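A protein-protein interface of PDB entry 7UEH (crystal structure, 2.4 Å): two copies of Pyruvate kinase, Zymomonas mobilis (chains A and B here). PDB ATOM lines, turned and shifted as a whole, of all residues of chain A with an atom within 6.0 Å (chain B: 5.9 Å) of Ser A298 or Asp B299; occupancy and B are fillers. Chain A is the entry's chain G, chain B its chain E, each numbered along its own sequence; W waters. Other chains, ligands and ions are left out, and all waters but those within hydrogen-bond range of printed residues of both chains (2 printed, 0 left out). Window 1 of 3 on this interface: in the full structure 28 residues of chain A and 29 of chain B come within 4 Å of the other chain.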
ATOM      1  N   THR A 293       3.652   6.474  16.135  1.00  0.00           N
ATOM      2  CA  THR A 293       4.159   5.610  17.192  1.00  0.00           C
ATOM      3  C   THR A 293       3.206   4.435  17.431  1.00  0.00           C
ATOM      4  O   THR A 293       2.074   4.399  16.942  1.00  0.00           O
ATOM      5  CB  THR A 293       4.346   6.356  18.509  1.00  0.00           C
ATOM      6  OG1 THR A 293       3.075   6.480  19.163  1.00  0.00           O
ATOM      7  CG2 THR A 293       5.044   7.761  18.304  1.00  0.00           C
ATOM      8  N   ARG A 294       3.686   3.452  18.192  1.00  0.00           N
ATOM      9  CA  ARG A 294       2.830   2.332  18.563  1.00  0.00           C
ATOM     10  C   ARG A 294       1.716   2.773  19.499  1.00  0.00           C
ATOM     11  O   ARG A 294       0.596   2.264  19.417  1.00  0.00           O
ATOM     12  CB  ARG A 294       3.628   1.232  19.243  1.00  0.00           C
ATOM     13  CG  ARG A 294       4.764   0.726  18.443  1.00  0.00           C
ATOM     14  CD  ARG A 294       4.261  -0.068  17.255  1.00  0.00           C
ATOM     15  NE  ARG A 294       5.430  -0.447  16.497  1.00  0.00           N
ATOM     16  CZ  ARG A 294       5.948   0.288  15.521  1.00  0.00           C
ATOM     17  NH1 ARG A 294       5.388   1.441  15.149  1.00  0.00           N
ATOM     18  NH2 ARG A 294       7.029  -0.139  14.918  1.00  0.00           N
ATOM     19  N   ALA A 295       2.005   3.692  20.422  1.00  0.00           N
ATOM     20  CA  ALA A 295       0.943   4.161  21.308  1.00  0.00           C
ATOM     21  C   ALA A 295      -0.178   4.782  20.505  1.00  0.00           C
ATOM     22  O   ALA A 295      -1.364   4.579  20.806  1.00  0.00           O
ATOM     23  CB  ALA A 295       1.483   5.167  22.316  1.00  0.00           C
ATOM     24  N   GLU A 296       0.188   5.526  19.459  1.00  0.00           N
ATOM     25  CA  GLU A 296      -0.793   6.283  18.700  1.00  0.00           C
ATOM     26  C   GLU A 296      -1.732   5.344  17.940  1.00  0.00           C
ATOM     27  O   GLU A 296      -2.947   5.545  17.931  1.00  0.00           O
ATOM     28  CB  GLU A 296      -0.051   7.258  17.774  1.00  0.00           C
ATOM     29  CG  GLU A 296       0.440   8.542  18.496  1.00  0.00           C
ATOM     30  CD  GLU A 296       1.602   9.326  17.808  1.00  0.00           C
ATOM     31  OE1 GLU A 296       2.026   8.987  16.699  1.00  0.00           O
ATOM     32  OE2 GLU A 296       2.106  10.310  18.396  1.00  0.00           O
ATOM     33  N   VAL A 297      -1.188   4.292  17.332  1.00  0.00           N
ATOM     34  CA  VAL A 297      -2.000   3.349  16.581  1.00  0.00           C
ATOM     35  C   VAL A 297      -2.910   2.588  17.526  1.00  0.00           C
ATOM     36  O   VAL A 297      -4.059   2.274  17.183  1.00  0.00           O
ATOM     37  CB  VAL A 297      -1.085   2.405  15.781  1.00  0.00           C
ATOM     38  CG1 VAL A 297      -1.819   1.154  15.357  1.00  0.00           C
ATOM     39  CG2 VAL A 297      -0.522   3.122  14.572  1.00  0.00           C
ATOM     40  N   SER A 298      -2.405   2.278  18.732  1.00  0.00           N
ATOM     41  CA  SER A 298      -3.213   1.639  19.766  1.00  0.00           C
ATOM     42  C   SER A 298      -4.361   2.539  20.186  1.00  0.00           C
ATOM     43  O   SER A 298      -5.493   2.071  20.381  1.00  0.00           O
ATOM     44  CB  SER A 298      -2.346   1.308  20.980  1.00  0.00           C
ATOM     45  OG  SER A 298      -3.144   1.001  22.112  1.00  0.00           O
ATOM     46  N   ASP A 299      -4.088   3.845  20.311  1.00  0.00           N
ATOM     47  CA  ASP A 299      -5.126   4.804  20.681  1.00  0.00           C
ATOM     48  C   ASP A 299      -6.260   4.825  19.669  1.00  0.00           C
ATOM     49  O   ASP A 299      -7.431   4.878  20.056  1.00  0.00           O
ATOM     50  CB  ASP A 299      -4.521   6.204  20.816  1.00  0.00           C
ATOM     51  CG  ASP A 299      -5.535   7.242  21.239  1.00  0.00           C
ATOM     52  OD1 ASP A 299      -6.299   6.965  22.183  1.00  0.00           O
ATOM     53  OD2 ASP A 299      -5.565   8.328  20.629  1.00  0.00           O
ATOM     54  N   VAL A 300      -5.934   4.855  18.362  1.00  0.00           N
ATOM     55  CA  VAL A 300      -6.988   4.901  17.345  1.00  0.00           C
ATOM     56  C   VAL A 300      -7.809   3.617  17.401  1.00  0.00           C
ATOM     57  O   VAL A 300      -9.043   3.641  17.402  1.00  0.00           O
ATOM     58  CB  VAL A 300      -6.404   5.103  15.935  1.00  0.00           C
ATOM     59  CG1 VAL A 300      -7.547   5.107  14.915  1.00  0.00           C
ATOM     60  CG2 VAL A 300      -5.638   6.390  15.807  1.00  0.00           C
ATOM     61  N   ALA A 301      -7.120   2.478  17.487  1.00  0.00           N
ATOM     62  CA  ALA A 301      -7.792   1.190  17.551  1.00  0.00           C
ATOM     63  C   ALA A 301      -8.669   1.072  18.799  1.00  0.00           C
ATOM     64  O   ALA A 301      -9.751   0.467  18.749  1.00  0.00           O
ATOM     65  CB  ALA A 301      -6.768   0.062  17.517  1.00  0.00           C
ATOM     66  N   ASN A 302      -8.239   1.651  19.923  1.00  0.00           N
ATOM     67  CA  ASN A 302      -9.037   1.480  21.130  1.00  0.00           C
ATOM     68  C   ASN A 302     -10.284   2.338  21.085  1.00  0.00           C
ATOM     69  O   ASN A 302     -11.300   1.954  21.662  1.00  0.00           O
ATOM     70  CB  ASN A 302      -8.234   1.757  22.396  1.00  0.00           C
ATOM     71  CG  ASN A 302      -7.590   0.497  22.947  1.00  0.00           C
ATOM     72  OD1 ASN A 302      -8.247  -0.365  23.486  1.00  0.00           O
ATOM     73  ND2 ASN A 302      -6.301   0.391  22.796  1.00  0.00           N
ATOM     74  N   ALA A 303     -10.250   3.454  20.362  1.00  0.00           N
ATOM     75  CA  ALA A 303     -11.477   4.202  20.103  1.00  0.00           C
ATOM     76  C   ALA A 303     -12.437   3.404  19.215  1.00  0.00           C
ATOM     77  O   ALA A 303     -13.663   3.417  19.427  1.00  0.00           O
ATOM     78  CB  ALA A 303     -11.135   5.536  19.457  1.00  0.00           C
ATOM     79  N   ARG B 246       6.184  -4.227  20.698  1.00  0.00           N
ATOM     80  CA  ARG B 246       5.458  -3.647  19.558  1.00  0.00           C
ATOM     81  C   ARG B 246       6.377  -2.930  18.586  1.00  0.00           C
ATOM     82  O   ARG B 246       6.107  -2.925  17.380  1.00  0.00           O
ATOM     83  CB  ARG B 246       4.346  -2.700  20.048  1.00  0.00           C
ATOM     84  CG  ARG B 246       3.243  -3.474  20.862  1.00  0.00           C
ATOM     85  CD  ARG B 246       2.157  -2.592  21.466  1.00  0.00           C
ATOM     86  NE  ARG B 246       2.670  -1.431  22.183  1.00  0.00           N
ATOM     87  CZ  ARG B 246       1.905  -0.468  22.676  1.00  0.00           C
ATOM     88  NH1 ARG B 246       0.576  -0.547  22.602  1.00  0.00           N
ATOM     89  NH2 ARG B 246       2.460   0.579  23.255  1.00  0.00           N
ATOM     90  N   PRO B 259      -2.652  -3.788  17.257  1.00  0.00           N
ATOM     91  CA  PRO B 259      -3.674  -3.752  18.319  1.00  0.00           C
ATOM     92  C   PRO B 259      -4.441  -5.065  18.430  1.00  0.00           C
ATOM     93  O   PRO B 259      -4.573  -5.621  19.543  1.00  0.00           O
ATOM     94  CB  PRO B 259      -4.577  -2.582  17.893  1.00  0.00           C
ATOM     95  CG  PRO B 259      -3.663  -1.687  17.127  1.00  0.00           C
ATOM     96  CD  PRO B 259      -2.776  -2.639  16.346  1.00  0.00           C
ATOM     97  N   GLN B 262      -2.099  -7.556  19.777  1.00  0.00           N
ATOM     98  CA  GLN B 262      -1.973  -7.301  21.207  1.00  0.00           C
ATOM     99  C   GLN B 262      -3.188  -7.838  21.987  1.00  0.00           C
ATOM    100  O   GLN B 262      -3.021  -8.523  22.990  1.00  0.00           O
ATOM    101  CB  GLN B 262      -1.764  -5.804  21.474  1.00  0.00           C
ATOM    102  CG  GLN B 262      -1.808  -5.492  22.963  1.00  0.00           C
ATOM    103  CD  GLN B 262      -1.383  -4.076  23.262  1.00  0.00           C
ATOM    104  OE1 GLN B 262      -0.714  -3.422  22.442  1.00  0.00           O
ATOM    105  NE2 GLN B 262      -1.776  -3.583  24.431  1.00  0.00           N
ATOM    106  N   VAL B 278       3.047  -5.169  28.130  1.00  0.00           N
ATOM    107  CA  VAL B 278       2.904  -4.401  26.898  1.00  0.00           C
ATOM    108  C   VAL B 278       4.061  -3.415  26.814  1.00  0.00           C
ATOM    109  O   VAL B 278       4.477  -2.828  27.822  1.00  0.00           O
ATOM    110  CB  VAL B 278       1.536  -3.700  26.858  1.00  0.00           C
ATOM    111  CG1 VAL B 278       1.428  -2.734  25.660  1.00  0.00           C
ATOM    112  CG2 VAL B 278       0.438  -4.742  26.809  1.00  0.00           C
ATOM    113  N   THR B 280       6.718  -0.599  24.316  1.00  0.00           N
ATOM    114  CA  THR B 280       7.226   0.252  23.246  1.00  0.00           C
ATOM    115  C   THR B 280       6.367   1.480  23.038  1.00  0.00           C
ATOM    116  O   THR B 280       5.192   1.373  22.680  1.00  0.00           O
ATOM    117  CB  THR B 280       7.382  -0.507  21.930  1.00  0.00           C
ATOM    118  OG1 THR B 280       8.487  -1.417  22.029  1.00  0.00           O
ATOM    119  CG2 THR B 280       7.671   0.450  20.807  1.00  0.00           C
ATOM    120  N   ALA B 281       6.973   2.649  23.262  1.00  0.00           N
ATOM    121  CA  ALA B 281       6.413   3.951  22.917  1.00  0.00           C
ATOM    122  C   ALA B 281       5.188   4.303  23.743  1.00  0.00           C
ATOM    123  O   ALA B 281       4.409   5.185  23.365  1.00  0.00           O
ATOM    124  CB  ALA B 281       6.070   4.020  21.422  1.00  0.00           C
ATOM    125  N   MET B 282       4.972   3.618  24.862  1.00  0.00           N
ATOM    126  CA  MET B 282       3.821   3.948  25.687  1.00  0.00           C
ATOM    127  C   MET B 282       3.817   5.423  26.066  1.00  0.00           C
ATOM    128  O   MET B 282       2.759   6.056  26.090  1.00  0.00           O
ATOM    129  CB  MET B 282       3.803   3.064  26.927  1.00  0.00           C
ATOM    130  CG  MET B 282       3.868   1.584  26.605  1.00  0.00           C
ATOM    131  SD  MET B 282       3.093   0.520  27.822  1.00  0.00           S
ATOM    132  CE  MET B 282       1.356   0.842  27.466  1.00  0.00           C
ATOM    133  N   LEU B 283       4.976   6.000  26.367  1.00  0.00           N
ATOM    134  CA  LEU B 283       5.013   7.439  26.625  1.00  0.00           C
ATOM    135  C   LEU B 283       6.077   8.128  25.773  1.00  0.00           C
ATOM    136  O   LEU B 283       6.848   8.971  26.239  1.00  0.00           O
ATOM    137  CB  LEU B 283       5.222   7.704  28.097  1.00  0.00           C
ATOM    138  CG  LEU B 283       4.176   7.235  29.097  1.00  0.00           C
ATOM    139  CD1 LEU B 283       4.574   7.752  30.424  1.00  0.00           C
ATOM    140  CD2 LEU B 283       2.728   7.639  28.773  1.00  0.00           C
ATOM    141  N   ARG B 294      -2.241  12.885  24.755  1.00  0.00           N
ATOM    142  CA  ARG B 294      -3.495  12.217  25.085  1.00  0.00           C
ATOM    143  C   ARG B 294      -3.527  10.801  24.536  1.00  0.00           C
ATOM    144  O   ARG B 294      -4.111   9.907  25.164  1.00  0.00           O
ATOM    145  CB  ARG B 294      -4.684  13.024  24.560  1.00  0.00           C
ATOM    146  CG  ARG B 294      -4.742  14.471  25.120  1.00  0.00           C
ATOM    147  CD  ARG B 294      -5.038  14.503  26.611  1.00  0.00           C
ATOM    148  NE  ARG B 294      -5.085  15.886  27.059  1.00  0.00           N
ATOM    149  CZ  ARG B 294      -4.007  16.598  27.382  1.00  0.00           C
ATOM    150  NH1 ARG B 294      -2.799  16.058  27.324  1.00  0.00           N
ATOM    151  NH2 ARG B 294      -4.137  17.858  27.753  1.00  0.00           N
ATOM    152  N   ALA B 295      -2.915  10.569  23.373  1.00  0.00           N
ATOM    153  CA  ALA B 295      -2.894   9.216  22.810  1.00  0.00           C
ATOM    154  C   ALA B 295      -2.023   8.286  23.646  1.00  0.00           C
ATOM    155  O   ALA B 295      -2.349   7.096  23.804  1.00  0.00           O
ATOM    156  CB  ALA B 295      -2.408   9.231  21.356  1.00  0.00           C
ATOM    157  N   GLU B 296      -0.954   8.823  24.233  1.00  0.00           N
ATOM    158  CA  GLU B 296      -0.083   8.007  25.069  1.00  0.00           C
ATOM    159  C   GLU B 296      -0.761   7.609  26.370  1.00  0.00           C
ATOM    160  O   GLU B 296      -0.602   6.467  26.828  1.00  0.00           O
ATOM    161  CB  GLU B 296       1.219   8.747  25.332  1.00  0.00           C
ATOM    162  CG  GLU B 296       2.101   8.708  24.087  1.00  0.00           C
ATOM    163  CD  GLU B 296       3.173   9.781  24.055  1.00  0.00           C
ATOM    164  OE1 GLU B 296       3.211  10.625  24.976  1.00  0.00           O
ATOM    165  OE2 GLU B 296       3.980   9.778  23.116  1.00  0.00           O
ATOM    166  N   VAL B 297      -1.517   8.512  26.994  1.00  0.00           N
ATOM    167  CA  VAL B 297      -2.155   8.108  28.240  1.00  0.00           C
ATOM    168  C   VAL B 297      -3.231   7.049  27.957  1.00  0.00           C
ATOM    169  O   VAL B 297      -3.386   6.085  28.712  1.00  0.00           O
ATOM    170  CB  VAL B 297      -2.701   9.340  28.968  1.00  0.00           C
ATOM    171  CG1 VAL B 297      -3.581   8.919  30.141  1.00  0.00           C
ATOM    172  CG2 VAL B 297      -1.528  10.152  29.449  1.00  0.00           C
ATOM    173  N   SER B 298      -3.925   7.175  26.819  1.00  0.00           N
ATOM    174  CA  SER B 298      -4.956   6.222  26.434  1.00  0.00           C
ATOM    175  C   SER B 298      -4.368   4.824  26.254  1.00  0.00           C
ATOM    176  O   SER B 298      -4.950   3.834  26.718  1.00  0.00           O
ATOM    177  CB  SER B 298      -5.637   6.691  25.147  1.00  0.00           C
ATOM    178  OG  SER B 298      -6.467   5.689  24.613  1.00  0.00           O
ATOM    179  N   ASP B 299      -3.213   4.735  25.592  1.00  0.00           N
ATOM    180  CA  ASP B 299      -2.544   3.458  25.338  1.00  0.00           C
ATOM    181  C   ASP B 299      -2.217   2.736  26.641  1.00  0.00           C
ATOM    182  O   ASP B 299      -2.461   1.530  26.774  1.00  0.00           O
ATOM    183  CB  ASP B 299      -1.271   3.717  24.504  1.00  0.00           C
ATOM    184  CG  ASP B 299      -0.478   2.455  24.200  1.00  0.00           C
ATOM    185  OD1 ASP B 299      -1.088   1.438  23.797  1.00  0.00           O
ATOM    186  OD2 ASP B 299       0.771   2.478  24.364  1.00  0.00           O
ATOM    187  N   VAL B 300      -1.657   3.460  27.616  1.00  0.00           N
ATOM    188  CA  VAL B 300      -1.389   2.860  28.921  1.00  0.00           C
ATOM    189  C   VAL B 300      -2.684   2.399  29.587  1.00  0.00           C
ATOM    190  O   VAL B 300      -2.776   1.274  30.098  1.00  0.00           O
ATOM    191  CB  VAL B 300      -0.626   3.848  29.816  1.00  0.00           C
ATOM    192  CG1 VAL B 300      -0.418   3.253  31.198  1.00  0.00           C
ATOM    193  CG2 VAL B 300       0.672   4.166  29.181  1.00  0.00           C
ATOM    194  N   ALA B 301      -3.680   3.284  29.667  1.00  0.00           N
ATOM    195  CA  ALA B 301      -4.948   2.882  30.278  1.00  0.00           C
ATOM    196  C   ALA B 301      -5.539   1.661  29.574  1.00  0.00           C
ATOM    197  O   ALA B 301      -6.013   0.749  30.237  1.00  0.00           O
ATOM    198  CB  ALA B 301      -5.956   4.028  30.260  1.00  0.00           C
ATOM    199  N   ASN B 302      -5.484   1.604  28.230  1.00  0.00           N
ATOM    200  CA  ASN B 302      -6.051   0.465  27.514  1.00  0.00           C
ATOM    201  C   ASN B 302      -5.258  -0.824  27.730  1.00  0.00           C
ATOM    202  O   ASN B 302      -5.838  -1.926  27.662  1.00  0.00           O
ATOM    203  CB  ASN B 302      -6.214   0.783  26.026  1.00  0.00           C
ATOM    204  CG  ASN B 302      -7.541   1.465  25.751  1.00  0.00           C
ATOM    205  OD1 ASN B 302      -8.596   0.882  25.960  1.00  0.00           O
ATOM    206  ND2 ASN B 302      -7.490   2.729  25.371  1.00  0.00           N
ATOM    207  N   ALA B 303      -3.962  -0.725  28.018  1.00  0.00           N
ATOM    208  CA  ALA B 303      -3.232  -1.911  28.436  1.00  0.00           C
ATOM    209  C   ALA B 303      -3.692  -2.370  29.797  1.00  0.00           C
ATOM    210  O   ALA B 303      -3.743  -3.572  30.063  1.00  0.00           O
ATOM    211  CB  ALA B 303      -1.734  -1.640  28.447  1.00  0.00           C
ATOM    212  N   ILE B 304      -4.046  -1.437  30.673  1.00  0.00           N
ATOM    213  CA  ILE B 304      -4.482  -1.832  32.004  1.00  0.00           C
ATOM    214  C   ILE B 304      -5.846  -2.522  31.935  1.00  0.00           C
ATOM    215  O   ILE B 304      -6.044  -3.590  32.539  1.00  0.00           O
ATOM    216  CB  ILE B 304      -4.489  -0.605  32.931  1.00  0.00           C
ATOM    217  CG1 ILE B 304      -3.039  -0.151  33.158  1.00  0.00           C
ATOM    218  CG2 ILE B 304      -5.213  -0.929  34.226  1.00  0.00           C
ATOM    219  CD1 ILE B 304      -2.883   1.166  33.902  1.00  0.00           C
HETATM  220  O   HOH W   1      -8.544  -1.781  26.316  1.00  0.00           O
HETATM  221  O   HOH W   2     -10.792   0.072  23.903  1.00  0.00           O
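Among the printed residues, pairs that only touch across the chains: Ala A295 with Ala B281, Asp A299 with Ala B295, Ala A295 with Asp B299, Ala A301 with Pro B259, Arg A294 with Thr B280, Val A297 with Pro B259 and Ser A298 with Arg B246.
Water W2 bridges OD1 of Asn A302 (2.6 Å) and OD1 of Asn B302 (3.1 Å).
Water W1 bridges OD1 of Asn B302 (2.7 Å) and OD1 of Asn A302 (3.2 Å).
Of the printed residues of chain B, Val A297 touches Pro B259 (3.8 Å).
Of chain B, only Arg B246 (3.8 Å) and Asp B299 (2.7 Å) come within 4 Å of Ser A298.
Printed residues of chain A within 4 Å of Arg B246: Arg A294 and Ser A298.
Printed residues of chain A within 4 Å of Ala B281: Ala A295 (3.1 Å).
Met B282 touches none of the printed residues of chain A.
Val B297 touches none of the printed residues of chain A.
The nearest printed residue of chain A that does not touch Ala B295 is Ala A295 (4.04 Å).
Ala A295 touches Asp B299, and with the chains exchanged Asp A299 touches Ala B295.
Ser A298 touches Asp B299, and with the chains exchanged Asp A299 touches Ser B298.
Asn B302 touches its own counterpart, Asn A302.
Positions printed for both chains: 294, 295, 296, 297, 298, 299, 300, 301, 302 and 303.
N of Ala A295 is in hydrogen-bond range of OG1 of Thr A293.
The backbone carbonyl oxygen (O) of Ser A298 is in hydrogen-bond range of the side-chain amide nitrogen (ND2) of Asn A302 (3.1 Å).
The guanidinium group (NH1) of Arg B246 lies close to the side-chain amide oxygen (OE1) of Gln B262 (3.2 Å).
The guanidinium group (NH2) of Arg B246 lies within hydrogen-bond range of the backbone carbonyl oxygen (O) of Thr B280 (2.9 Å).
The side-chain carboxylate of Asp B299 lies within salt-bridge range of the guanidinium group of Arg B246 (2.8 Å).
O of Ser B298 lies within hydrogen-bond range of ND2 of Asn B302, at 3.1 Å.
The backbone carbonyl oxygen (O) of Arg B246 lies within hydrogen-bond range of the guanidinium group (NE) of Arg A294 (2.7 Å).
OG of Ser A298 lies within hydrogen-bond range of OD1 of Asp B299, 2.7 Å away.
OG of Ser B298 is in hydrogen-bond range of OD1 of Asp A299.
OD1 of Asn A302 lies close to OD1 of Asn B302, at 2.8 Å.
Of the 11 printed residues of chain A, 7 touch a printed residue of chain B.
Printed residues of chain A that touch a printed residue of chain B: Arg A294, Ala A295, Val A297, Ser A298, Asp A299, Ala A301 and Asn A302.
Hydrophobic or aromatic side chains of chain A within 4 Å of the printed part of chain B: Ala A295, Val A297 and Ala A301.
Hydrophobic or aromatic side chains of chain B that line the printed part of chain A: Pro B259 and Ala B295.
Among the printed residues, no Asp or Glu carboxylate lies within 4 Å of a Lys or Arg side-chain nitrogen of the other chain.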
